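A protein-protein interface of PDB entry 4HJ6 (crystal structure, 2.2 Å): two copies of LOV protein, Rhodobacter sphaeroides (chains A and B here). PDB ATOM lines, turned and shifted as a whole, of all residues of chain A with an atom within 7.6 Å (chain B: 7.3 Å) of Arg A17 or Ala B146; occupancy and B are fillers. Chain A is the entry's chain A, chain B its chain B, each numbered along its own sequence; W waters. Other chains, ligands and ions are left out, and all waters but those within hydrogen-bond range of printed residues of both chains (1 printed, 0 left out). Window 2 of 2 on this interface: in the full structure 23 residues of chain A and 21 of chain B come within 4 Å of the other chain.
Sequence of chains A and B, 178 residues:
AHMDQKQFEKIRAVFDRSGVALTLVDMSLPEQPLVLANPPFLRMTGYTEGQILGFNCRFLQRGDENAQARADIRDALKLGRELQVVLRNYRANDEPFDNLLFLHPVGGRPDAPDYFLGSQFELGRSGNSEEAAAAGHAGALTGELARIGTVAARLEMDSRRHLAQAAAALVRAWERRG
NH2 of Arg A17 is in hydrogen-bond range of O of Ala B146 (3.5 Å).
The backbone NH (N) of Gly A19 lies within hydrogen-bond range of the side-chain carboxylate (OE1) of Glu B156, at 3.1 Å.
The guanidinium group of Arg B147 is in salt-bridge range of the side-chain carboxylate of Glu A144.
OE2 of Glu B144 is in salt-bridge range of NH1 of Arg A147, at 2.6 Å.
The guanidinium group (NE) of Arg B147 lies close to the guanidinium group (NE) of Arg A147 (3.0 Å).
Glu A144 touches Arg B147, and with the chains exchanged Arg A147 touches Glu B144.
Arg A147 touches its own counterpart, Arg B147.
Of the 7 pairs that touch across the chains among the printed residues, 3 have their exchanged pair printed and touching as well.
Water W1 lies within hydrogen-bond range of the backbone carbonyl oxygen of Ala B140 (2.6 Å) and the guanidinium group of Arg A147 (3.2 Å).
Val A14 touches none of the printed residues of chain B.
Arg A17 touches two residues of chain B.
Printed residues of chain B within 4 Å of Ser A18: Glu B156 (3.99 Å).
Of the printed residues of chain B, Glu A144 touches Arg B147.
Of the printed residues of chain B, Arg A147 touches Glu B144 (2.6 Å) and Arg B147 (3.0 Å).
Gly B143 touches none of the printed residues of chain A.
Ala B146 touches one residue of chain A.
Printed residues of chain A within 4 Å of Glu B156: Ser A18 (3.99 Å) and Gly A19 (3.1 Å).
The nearest residue of chain B that does not touch Arg A17 is Lys B10 (4.1 Å).
Among the printed residues, merely in contact across the chains: Arg A17 with Arg B147 (3.3 Å) and Ser A18 with Glu B156 (3.99 Å).
Printed residues of chain B that touch a printed residue of chain A: Glu B144, Ala B146, Arg B147 and Glu B156.
Among the printed residues, 7 pairs touch across the chains.
Among the printed residues, Asp or Glu carboxylates within 4 Å of a Lys or Arg side-chain nitrogen of the other chain: Glu A144 with Arg B147 (3.0 Å) and Arg A147 with Glu B144 (2.6 Å).
The side-chain hydroxyl (OG) of Ser A18 is in hydrogen-bond range of the backbone NH (N) of Val A20.
The side-chain hydroxyl (OG) of Ser A18 sits at hydrogen-bond distance from the side-chain carboxylate (OE2) of Glu A144.
The guanidinium group (NH2) of Arg A147 is in salt-bridge range of the side-chain carboxylate (OE1) of Glu A144 (2.6 Å).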
ATOM      1  N   ILE A  11       9.887 -36.228   3.261  1.00  0.00           N
ATOM      2  CA  ILE A  11      10.039 -35.417   2.053  1.00  0.00           C
ATOM      3  C   ILE A  11       8.901 -34.412   1.954  1.00  0.00           C
ATOM      4  O   ILE A  11       9.122 -33.242   1.632  1.00  0.00           O
ATOM      5  CB  ILE A  11      10.107 -36.287   0.771  1.00  0.00           C
ATOM      6  CG1 ILE A  11      11.398 -37.115   0.762  1.00  0.00           C
ATOM      7  CG2 ILE A  11      10.015 -35.424  -0.500  1.00  0.00           C
ATOM      8  CD1 ILE A  11      11.603 -37.939  -0.506  1.00  0.00           C
ATOM      9  N   ARG A  12       7.689 -34.856   2.269  1.00  0.00           N
ATOM     10  CA  ARG A  12       6.531 -33.978   2.211  1.00  0.00           C
ATOM     11  C   ARG A  12       6.728 -32.800   3.165  1.00  0.00           C
ATOM     12  O   ARG A  12       6.507 -31.653   2.788  1.00  0.00           O
ATOM     13  CB  ARG A  12       5.246 -34.755   2.535  1.00  0.00           C
ATOM     14  CG  ARG A  12       3.960 -34.036   2.133  1.00  0.00           C
ATOM     15  CD  ARG A  12       2.698 -34.793   2.576  1.00  0.00           C
ATOM     16  NE  ARG A  12       2.461 -36.028   1.824  1.00  0.00           N
ATOM     17  CZ  ARG A  12       1.700 -36.104   0.732  1.00  0.00           C
ATOM     18  NH1 ARG A  12       1.525 -37.266   0.111  1.00  0.00           N
ATOM     19  NH2 ARG A  12       1.117 -35.012   0.259  1.00  0.00           N
ATOM     20  N   ALA A  13       7.164 -33.088   4.388  1.00  0.00           N
ATOM     21  CA  ALA A  13       7.433 -32.049   5.392  1.00  0.00           C
ATOM     22  C   ALA A  13       8.415 -30.994   4.869  1.00  0.00           C
ATOM     23  O   ALA A  13       8.156 -29.789   4.950  1.00  0.00           O
ATOM     24  CB  ALA A  13       7.974 -32.683   6.678  1.00  0.00           C
ATOM     25  N   VAL A  14       9.540 -31.469   4.341  1.00  0.00           N
ATOM     26  CA  VAL A  14      10.555 -30.617   3.739  1.00  0.00           C
ATOM     27  C   VAL A  14       9.966 -29.760   2.636  1.00  0.00           C
ATOM     28  O   VAL A  14      10.292 -28.575   2.522  1.00  0.00           O
ATOM     29  CB  VAL A  14      11.713 -31.468   3.171  1.00  0.00           C
ATOM     30  CG1 VAL A  14      12.653 -30.624   2.312  1.00  0.00           C
ATOM     31  CG2 VAL A  14      12.468 -32.141   4.299  1.00  0.00           C
ATOM     32  N   PHE A  15       9.084 -30.346   1.830  1.00  0.00           N
ATOM     33  CA  PHE A  15       8.463 -29.614   0.731  1.00  0.00           C
ATOM     34  C   PHE A  15       7.559 -28.476   1.217  1.00  0.00           C
ATOM     35  O   PHE A  15       7.599 -27.368   0.662  1.00  0.00           O
ATOM     36  CB  PHE A  15       7.676 -30.575  -0.182  1.00  0.00           C
ATOM     37  CG  PHE A  15       8.472 -31.106  -1.354  1.00  0.00           C
ATOM     38  CD1 PHE A  15       9.752 -31.619  -1.175  1.00  0.00           C
ATOM     39  CD2 PHE A  15       7.928 -31.106  -2.638  1.00  0.00           C
ATOM     40  CE1 PHE A  15      10.488 -32.105  -2.255  1.00  0.00           C
ATOM     41  CE2 PHE A  15       8.660 -31.600  -3.730  1.00  0.00           C
ATOM     42  CZ  PHE A  15       9.934 -32.099  -3.534  1.00  0.00           C
ATOM     43  N   ASP A  16       6.749 -28.744   2.241  1.00  0.00           N
ATOM     44  CA  ASP A  16       5.777 -27.757   2.722  1.00  0.00           C
ATOM     45  C   ASP A  16       6.452 -26.533   3.341  1.00  0.00           C
ATOM     46  O   ASP A  16       5.991 -25.403   3.167  1.00  0.00           O
ATOM     47  CB  ASP A  16       4.830 -28.385   3.749  1.00  0.00           C
ATOM     48  CG  ASP A  16       4.200 -29.673   3.256  1.00  0.00           C
ATOM     49  OD1 ASP A  16       3.814 -29.738   2.071  1.00  0.00           O
ATOM     50  OD2 ASP A  16       4.086 -30.624   4.063  1.00  0.00           O
ATOM     51  N   ARG A  17       7.554 -26.779   4.045  1.00  0.00           N
ATOM     52  CA  ARG A  17       8.277 -25.756   4.802  1.00  0.00           C
ATOM     53  C   ARG A  17       9.258 -24.939   3.954  1.00  0.00           C
ATOM     54  O   ARG A  17       9.493 -23.759   4.225  1.00  0.00           O
ATOM     55  CB  ARG A  17       9.007 -26.425   5.981  1.00  0.00           C
ATOM     56  CG  ARG A  17      10.426 -25.938   6.234  1.00  0.00           C
ATOM     57  CD  ARG A  17      10.493 -24.984   7.422  1.00  0.00           C
ATOM     58  NE  ARG A  17      10.306 -25.667   8.706  1.00  0.00           N
ATOM     59  CZ  ARG A  17      10.001 -25.052   9.848  1.00  0.00           C
ATOM     60  NH1 ARG A  17       9.852 -25.748  10.970  1.00  0.00           N
ATOM     61  NH2 ARG A  17       9.837 -23.733   9.864  1.00  0.00           N
ATOM     62  N   SER A  18       9.797 -25.559   2.910  1.00  0.00           N
ATOM     63  CA  SER A  18      10.910 -24.987   2.142  1.00  0.00           C
ATOM     64  C   SER A  18      10.639 -23.638   1.478  1.00  0.00           C
ATOM     65  O   SER A  18       9.514 -23.333   1.102  1.00  0.00           O
ATOM     66  CB  SER A  18      11.367 -25.970   1.068  1.00  0.00           C
ATOM     67  OG  SER A  18      12.448 -25.431   0.327  1.00  0.00           O
ATOM     68  N   GLY A  19      11.693 -22.843   1.317  1.00  0.00           N
ATOM     69  CA  GLY A  19      11.580 -21.574   0.632  1.00  0.00           C
ATOM     70  C   GLY A  19      12.111 -21.569  -0.794  1.00  0.00           C
ATOM     71  O   GLY A  19      12.345 -20.493  -1.356  1.00  0.00           O
ATOM     72  N   VAL A  20      12.333 -22.746  -1.380  1.00  0.00           N
ATOM     73  CA  VAL A  20      12.635 -22.812  -2.815  1.00  0.00           C
ATOM     74  C   VAL A  20      11.562 -23.652  -3.491  1.00  0.00           C
ATOM     75  O   VAL A  20      10.975 -24.538  -2.859  1.00  0.00           O
ATOM     76  CB  VAL A  20      14.021 -23.432  -3.115  1.00  0.00           C
ATOM     77  CG1 VAL A  20      15.153 -22.490  -2.693  1.00  0.00           C
ATOM     78  CG2 VAL A  20      14.169 -24.794  -2.419  1.00  0.00           C
ATOM     79  N   LEU A  22      10.075 -26.584  -5.236  1.00  0.00           N
ATOM     80  CA  LEU A  22      10.464 -27.991  -5.258  1.00  0.00           C
ATOM     81  C   LEU A  22       9.341 -28.806  -5.926  1.00  0.00           C
ATOM     82  O   LEU A  22       8.159 -28.541  -5.686  1.00  0.00           O
ATOM     83  CB  LEU A  22      10.706 -28.495  -3.840  1.00  0.00           C
ATOM     84  CG  LEU A  22      11.886 -27.926  -3.038  1.00  0.00           C
ATOM     85  CD1 LEU A  22      11.814 -28.396  -1.592  1.00  0.00           C
ATOM     86  CD2 LEU A  22      13.214 -28.363  -3.639  1.00  0.00           C
ATOM     87  N   ASN A  38       5.411 -27.881  -4.345  1.00  0.00           N
ATOM     88  CA  ASN A  38       5.296 -27.035  -3.154  1.00  0.00           C
ATOM     89  C   ASN A  38       4.836 -25.591  -3.449  1.00  0.00           C
ATOM     90  O   ASN A  38       4.865 -25.157  -4.600  1.00  0.00           O
ATOM     91  CB  ASN A  38       6.599 -27.083  -2.353  1.00  0.00           C
ATOM     92  CG  ASN A  38       7.665 -26.156  -2.894  1.00  0.00           C
ATOM     93  OD1 ASN A  38       7.603 -25.699  -4.035  1.00  0.00           O
ATOM     94  ND2 ASN A  38       8.671 -25.881  -2.066  1.00  0.00           N
ATOM     95  N   PRO A  39       4.387 -24.850  -2.414  1.00  0.00           N
ATOM     96  CA  PRO A  39       3.838 -23.507  -2.678  1.00  0.00           C
ATOM     97  C   PRO A  39       4.721 -22.520  -3.465  1.00  0.00           C
ATOM     98  O   PRO A  39       4.176 -21.842  -4.338  1.00  0.00           O
ATOM     99  CB  PRO A  39       3.518 -22.980  -1.276  1.00  0.00           C
ATOM    100  CG  PRO A  39       3.158 -24.226  -0.524  1.00  0.00           C
ATOM    101  CD  PRO A  39       4.128 -25.276  -1.026  1.00  0.00           C
ATOM    102  N   PRO A  40       6.039 -22.436  -3.179  1.00  0.00           N
ATOM    103  CA  PRO A  40       6.816 -21.525  -4.039  1.00  0.00           C
ATOM    104  C   PRO A  40       6.762 -21.942  -5.523  1.00  0.00           C
ATOM    105  O   PRO A  40       6.803 -21.078  -6.404  1.00  0.00           O
ATOM    106  CB  PRO A  40       8.247 -21.613  -3.487  1.00  0.00           C
ATOM    107  CG  PRO A  40       8.227 -22.638  -2.392  1.00  0.00           C
ATOM    108  CD  PRO A  40       6.813 -22.935  -2.024  1.00  0.00           C
ATOM    109  N   GLU A 144      17.988 -28.301   1.780  1.00  0.00           N
ATOM    110  CA  GLU A 144      16.827 -29.194   1.685  1.00  0.00           C
ATOM    111  C   GLU A 144      17.215 -30.626   1.315  1.00  0.00           C
ATOM    112  O   GLU A 144      16.665 -31.578   1.858  1.00  0.00           O
ATOM    113  CB  GLU A 144      15.791 -28.659   0.679  1.00  0.00           C
ATOM    114  CG  GLU A 144      15.502 -27.151   0.742  1.00  0.00           C
ATOM    115  CD  GLU A 144      14.787 -26.704   2.024  1.00  0.00           C
ATOM    116  OE1 GLU A 144      14.815 -27.434   3.046  1.00  0.00           O
ATOM    117  OE2 GLU A 144      14.212 -25.588   2.014  1.00  0.00           O
ATOM    118  N   ARG A 147      18.375 -32.389   4.385  1.00  0.00           N
ATOM    119  CA  ARG A 147      17.287 -32.780   5.293  1.00  0.00           C
ATOM    120  C   ARG A 147      16.515 -34.001   4.789  1.00  0.00           C
ATOM    121  O   ARG A 147      15.998 -34.791   5.579  1.00  0.00           O
ATOM    122  CB  ARG A 147      16.323 -31.610   5.556  1.00  0.00           C
ATOM    123  CG  ARG A 147      16.951 -30.476   6.361  1.00  0.00           C
ATOM    124  CD  ARG A 147      16.041 -29.256   6.468  1.00  0.00           C
ATOM    125  NE  ARG A 147      16.800 -28.086   6.912  1.00  0.00           N
ATOM    126  CZ  ARG A 147      17.036 -26.996   6.178  1.00  0.00           C
ATOM    127  NH1 ARG A 147      17.762 -26.003   6.693  1.00  0.00           N
ATOM    128  NH2 ARG A 147      16.549 -26.887   4.944  1.00  0.00           N
ATOM    129  N   LYS B  10      14.695 -26.220  19.726  1.00  0.00           N
ATOM    130  CA  LYS B  10      14.618 -26.255  18.266  1.00  0.00           C
ATOM    131  C   LYS B  10      15.867 -25.608  17.666  1.00  0.00           C
ATOM    132  O   LYS B  10      16.492 -26.151  16.757  1.00  0.00           O
ATOM    133  CB  LYS B  10      13.360 -25.526  17.789  1.00  0.00           C
ATOM    134  CG  LYS B  10      13.290 -25.288  16.288  1.00  0.00           C
ATOM    135  CD  LYS B  10      13.111 -26.582  15.499  1.00  0.00           C
ATOM    136  CE  LYS B  10      12.714 -26.290  14.045  1.00  0.00           C
ATOM    137  NZ  LYS B  10      12.719 -27.529  13.211  1.00  0.00           N
ATOM    138  N   ALA B 140      21.960 -21.013   2.168  1.00  0.00           N
ATOM    139  CA  ALA B 140      21.886 -22.039   3.196  1.00  0.00           C
ATOM    140  C   ALA B 140      21.514 -21.403   4.534  1.00  0.00           C
ATOM    141  O   ALA B 140      20.635 -21.906   5.239  1.00  0.00           O
ATOM    142  CB  ALA B 140      23.221 -22.780   3.317  1.00  0.00           C
ATOM    143  N   LEU B 141      22.196 -20.317   4.895  1.00  0.00           N
ATOM    144  CA  LEU B 141      21.884 -19.598   6.129  1.00  0.00           C
ATOM    145  C   LEU B 141      20.412 -19.213   6.193  1.00  0.00           C
ATOM    146  O   LEU B 141      19.752 -19.423   7.219  1.00  0.00           O
ATOM    147  CB  LEU B 141      22.736 -18.331   6.253  1.00  0.00           C
ATOM    148  CG  LEU B 141      22.414 -17.414   7.450  1.00  0.00           C
ATOM    149  CD1 LEU B 141      22.574 -18.139   8.795  1.00  0.00           C
ATOM    150  CD2 LEU B 141      23.298 -16.181   7.437  1.00  0.00           C
ATOM    151  N   THR B 142      19.896 -18.646   5.103  1.00  0.00           N
ATOM    152  CA  THR B 142      18.516 -18.162   5.090  1.00  0.00           C
ATOM    153  C   THR B 142      17.566 -19.330   5.309  1.00  0.00           C
ATOM    154  O   THR B 142      16.515 -19.182   5.952  1.00  0.00           O
ATOM    155  CB  THR B 142      18.177 -17.426   3.774  1.00  0.00           C
ATOM    156  OG1 THR B 142      19.156 -16.407   3.547  1.00  0.00           O
ATOM    157  CG2 THR B 142      16.817 -16.754   3.870  1.00  0.00           C
ATOM    158  N   GLY B 143      17.943 -20.499   4.797  1.00  0.00           N
ATOM    159  CA  GLY B 143      17.174 -21.701   5.063  1.00  0.00           C
ATOM    160  C   GLY B 143      17.131 -22.012   6.549  1.00  0.00           C
ATOM    161  O   GLY B 143      16.083 -22.387   7.080  1.00  0.00           O
ATOM    162  N   GLU B 144      18.273 -21.877   7.227  1.00  0.00           N
ATOM    163  CA  GLU B 144      18.324 -22.177   8.651  1.00  0.00           C
ATOM    164  C   GLU B 144      17.559 -21.129   9.463  1.00  0.00           C
ATOM    165  O   GLU B 144      16.874 -21.462  10.425  1.00  0.00           O
ATOM    166  CB  GLU B 144      19.786 -22.297   9.108  1.00  0.00           C
ATOM    167  CG  GLU B 144      20.550 -23.426   8.382  1.00  0.00           C
ATOM    168  CD  GLU B 144      20.290 -24.782   9.013  1.00  0.00           C
ATOM    169  OE1 GLU B 144      20.739 -24.978  10.162  1.00  0.00           O
ATOM    170  OE2 GLU B 144      19.670 -25.659   8.392  1.00  0.00           O
ATOM    171  N   LEU B 145      17.683 -19.865   9.073  1.00  0.00           N
ATOM    172  CA  LEU B 145      16.953 -18.793   9.737  1.00  0.00           C
ATOM    173  C   LEU B 145      15.462 -19.065   9.685  1.00  0.00           C
ATOM    174  O   LEU B 145      14.761 -18.891  10.682  1.00  0.00           O
ATOM    175  CB  LEU B 145      17.249 -17.436   9.083  1.00  0.00           C
ATOM    176  CG  LEU B 145      18.672 -16.935   9.304  1.00  0.00           C
ATOM    177  CD1 LEU B 145      18.903 -15.646   8.510  1.00  0.00           C
ATOM    178  CD2 LEU B 145      18.942 -16.717  10.796  1.00  0.00           C
ATOM    179  N   ALA B 146      14.984 -19.498   8.522  1.00  0.00           N
ATOM    180  CA  ALA B 146      13.564 -19.765   8.337  1.00  0.00           C
ATOM    181  C   ALA B 146      13.100 -20.943   9.176  1.00  0.00           C
ATOM    182  O   ALA B 146      11.936 -21.000   9.577  1.00  0.00           O
ATOM    183  CB  ALA B 146      13.243 -19.993   6.860  1.00  0.00           C
ATOM    184  N   ARG B 147      13.990 -21.892   9.445  1.00  0.00           N
ATOM    185  CA  ARG B 147      13.620 -23.007  10.305  1.00  0.00           C
ATOM    186  C   ARG B 147      13.512 -22.556  11.751  1.00  0.00           C
ATOM    187  O   ARG B 147      12.739 -23.097  12.526  1.00  0.00           O
ATOM    188  CB  ARG B 147      14.614 -24.158  10.185  1.00  0.00           C
ATOM    189  CG  ARG B 147      14.061 -25.351   9.449  1.00  0.00           C
ATOM    190  CD  ARG B 147      14.783 -25.562   8.146  1.00  0.00           C
ATOM    191  NE  ARG B 147      14.183 -26.653   7.382  1.00  0.00           N
ATOM    192  CZ  ARG B 147      13.722 -26.534   6.139  1.00  0.00           C
ATOM    193  NH1 ARG B 147      13.189 -27.585   5.529  1.00  0.00           N
ATOM    194  NH2 ARG B 147      13.799 -25.368   5.500  1.00  0.00           N
ATOM    195  N   ILE B 148      14.301 -21.555  12.112  1.00  0.00           N
ATOM    196  CA  ILE B 148      14.315 -21.070  13.482  1.00  0.00           C
ATOM    197  C   ILE B 148      13.071 -20.238  13.718  1.00  0.00           C
ATOM    198  O   ILE B 148      12.409 -20.384  14.742  1.00  0.00           O
ATOM    199  CB  ILE B 148      15.578 -20.248  13.775  1.00  0.00           C
ATOM    200  CG1 ILE B 148      16.793 -21.175  13.856  1.00  0.00           C
ATOM    201  CG2 ILE B 148      15.429 -19.463  15.065  1.00  0.00           C
ATOM    202  CD1 ILE B 148      18.105 -20.448  14.096  1.00  0.00           C
ATOM    203  N   GLY B 149      12.751 -19.372  12.761  1.00  0.00           N
ATOM    204  CA  GLY B 149      11.553 -18.558  12.840  1.00  0.00           C
ATOM    205  C   GLY B 149      11.851 -17.078  12.711  1.00  0.00           C
ATOM    206  O   GLY B 149      10.938 -16.270  12.546  1.00  0.00           O
ATOM    207  N   THR B 150      13.131 -16.720  12.771  1.00  0.00           N
ATOM    208  CA  THR B 150      13.527 -15.311  12.742  1.00  0.00           C
ATOM    209  C   THR B 150      13.238 -14.647  11.385  1.00  0.00           C
ATOM    210  O   THR B 150      12.963 -13.443  11.314  1.00  0.00           O
ATOM    211  CB  THR B 150      15.016 -15.115  13.161  1.00  0.00           C
ATOM    212  OG1 THR B 150      15.884 -15.472  12.081  1.00  0.00           O
ATOM    213  CG2 THR B 150      15.333 -15.977  14.351  1.00  0.00           C
ATOM    214  N   VAL B 151      13.306 -15.438  10.319  1.00  0.00           N
ATOM    215  CA  VAL B 151      12.885 -14.984   8.988  1.00  0.00           C
ATOM    216  C   VAL B 151      11.496 -15.566   8.657  1.00  0.00           C
ATOM    217  O   VAL B 151      11.330 -16.796   8.620  1.00  0.00           O
ATOM    218  CB  VAL B 151      13.919 -15.390   7.902  1.00  0.00           C
ATOM    219  CG1 VAL B 151      13.275 -15.403   6.494  1.00  0.00           C
ATOM    220  CG2 VAL B 151      15.143 -14.455   7.938  1.00  0.00           C
ATOM    221  N   ALA B 152      10.502 -14.700   8.440  1.00  0.00           N
ATOM    222  CA  ALA B 152       9.141 -15.165   8.117  1.00  0.00           C
ATOM    223  C   ALA B 152       9.183 -16.124   6.927  1.00  0.00           C
ATOM    224  O   ALA B 152       9.872 -15.850   5.945  1.00  0.00           O
ATOM    225  CB  ALA B 152       8.216 -13.993   7.821  1.00  0.00           C
ATOM    226  N   ALA B 153       8.480 -17.253   7.024  1.00  0.00           N
ATOM    227  CA  ALA B 153       8.505 -18.264   5.964  1.00  0.00           C
ATOM    228  C   ALA B 153       8.224 -17.676   4.565  1.00  0.00           C
ATOM    229  O   ALA B 153       8.936 -17.978   3.593  1.00  0.00           O
ATOM    230  CB  ALA B 153       7.514 -19.382   6.276  1.00  0.00           C
ATOM    231  N   ARG B 154       7.195 -16.835   4.466  1.00  0.00           N
ATOM    232  CA  ARG B 154       6.804 -16.260   3.172  1.00  0.00           C
ATOM    233  C   ARG B 154       7.914 -15.366   2.591  1.00  0.00           C
ATOM    234  O   ARG B 154       7.983 -15.163   1.372  1.00  0.00           O
ATOM    235  CB  ARG B 154       5.497 -15.475   3.317  1.00  0.00           C
ATOM    236  CG  ARG B 154       4.987 -14.866   2.023  1.00  0.00           C
ATOM    237  CD  ARG B 154       4.850 -15.922   0.939  1.00  0.00           C
ATOM    238  NE  ARG B 154       4.373 -15.361  -0.327  1.00  0.00           N
ATOM    239  CZ  ARG B 154       5.171 -14.959  -1.314  1.00  0.00           C
ATOM    240  NH1 ARG B 154       6.485 -15.073  -1.181  1.00  0.00           N
ATOM    241  NH2 ARG B 154       4.653 -14.452  -2.433  1.00  0.00           N
ATOM    242  N   LEU B 155       8.794 -14.868   3.467  1.00  0.00           N
ATOM    243  CA  LEU B 155       9.828 -13.908   3.077  1.00  0.00           C
ATOM    244  C   LEU B 155      11.186 -14.574   2.875  1.00  0.00           C
ATOM    245  O   LEU B 155      12.177 -13.888   2.636  1.00  0.00           O
ATOM    246  CB  LEU B 155       9.990 -12.813   4.136  1.00  0.00           C
ATOM    247  CG  LEU B 155       8.850 -11.855   4.468  1.00  0.00           C
ATOM    248  CD1 LEU B 155       9.299 -10.866   5.540  1.00  0.00           C
ATOM    249  CD2 LEU B 155       8.401 -11.134   3.216  1.00  0.00           C
ATOM    250  N   GLU B 156      11.239 -15.897   2.991  1.00  0.00           N
ATOM    251  CA  GLU B 156      12.501 -16.610   2.833  1.00  0.00           C
ATOM    252  C   GLU B 156      13.190 -16.278   1.504  1.00  0.00           C
ATOM    253  O   GLU B 156      14.367 -15.904   1.493  1.00  0.00           O
ATOM    254  CB  GLU B 156      12.338 -18.129   2.995  1.00  0.00           C
ATOM    255  CG  GLU B 156      13.701 -18.834   3.030  1.00  0.00           C
ATOM    256  CD  GLU B 156      13.623 -20.345   3.192  1.00  0.00           C
ATOM    257  OE1 GLU B 156      12.551 -20.855   3.603  1.00  0.00           O
ATOM    258  OE2 GLU B 156      14.651 -21.019   2.914  1.00  0.00           O
HETATM  259  O   HOH W   1      19.846 -24.406   4.865  1.00  0.00           O
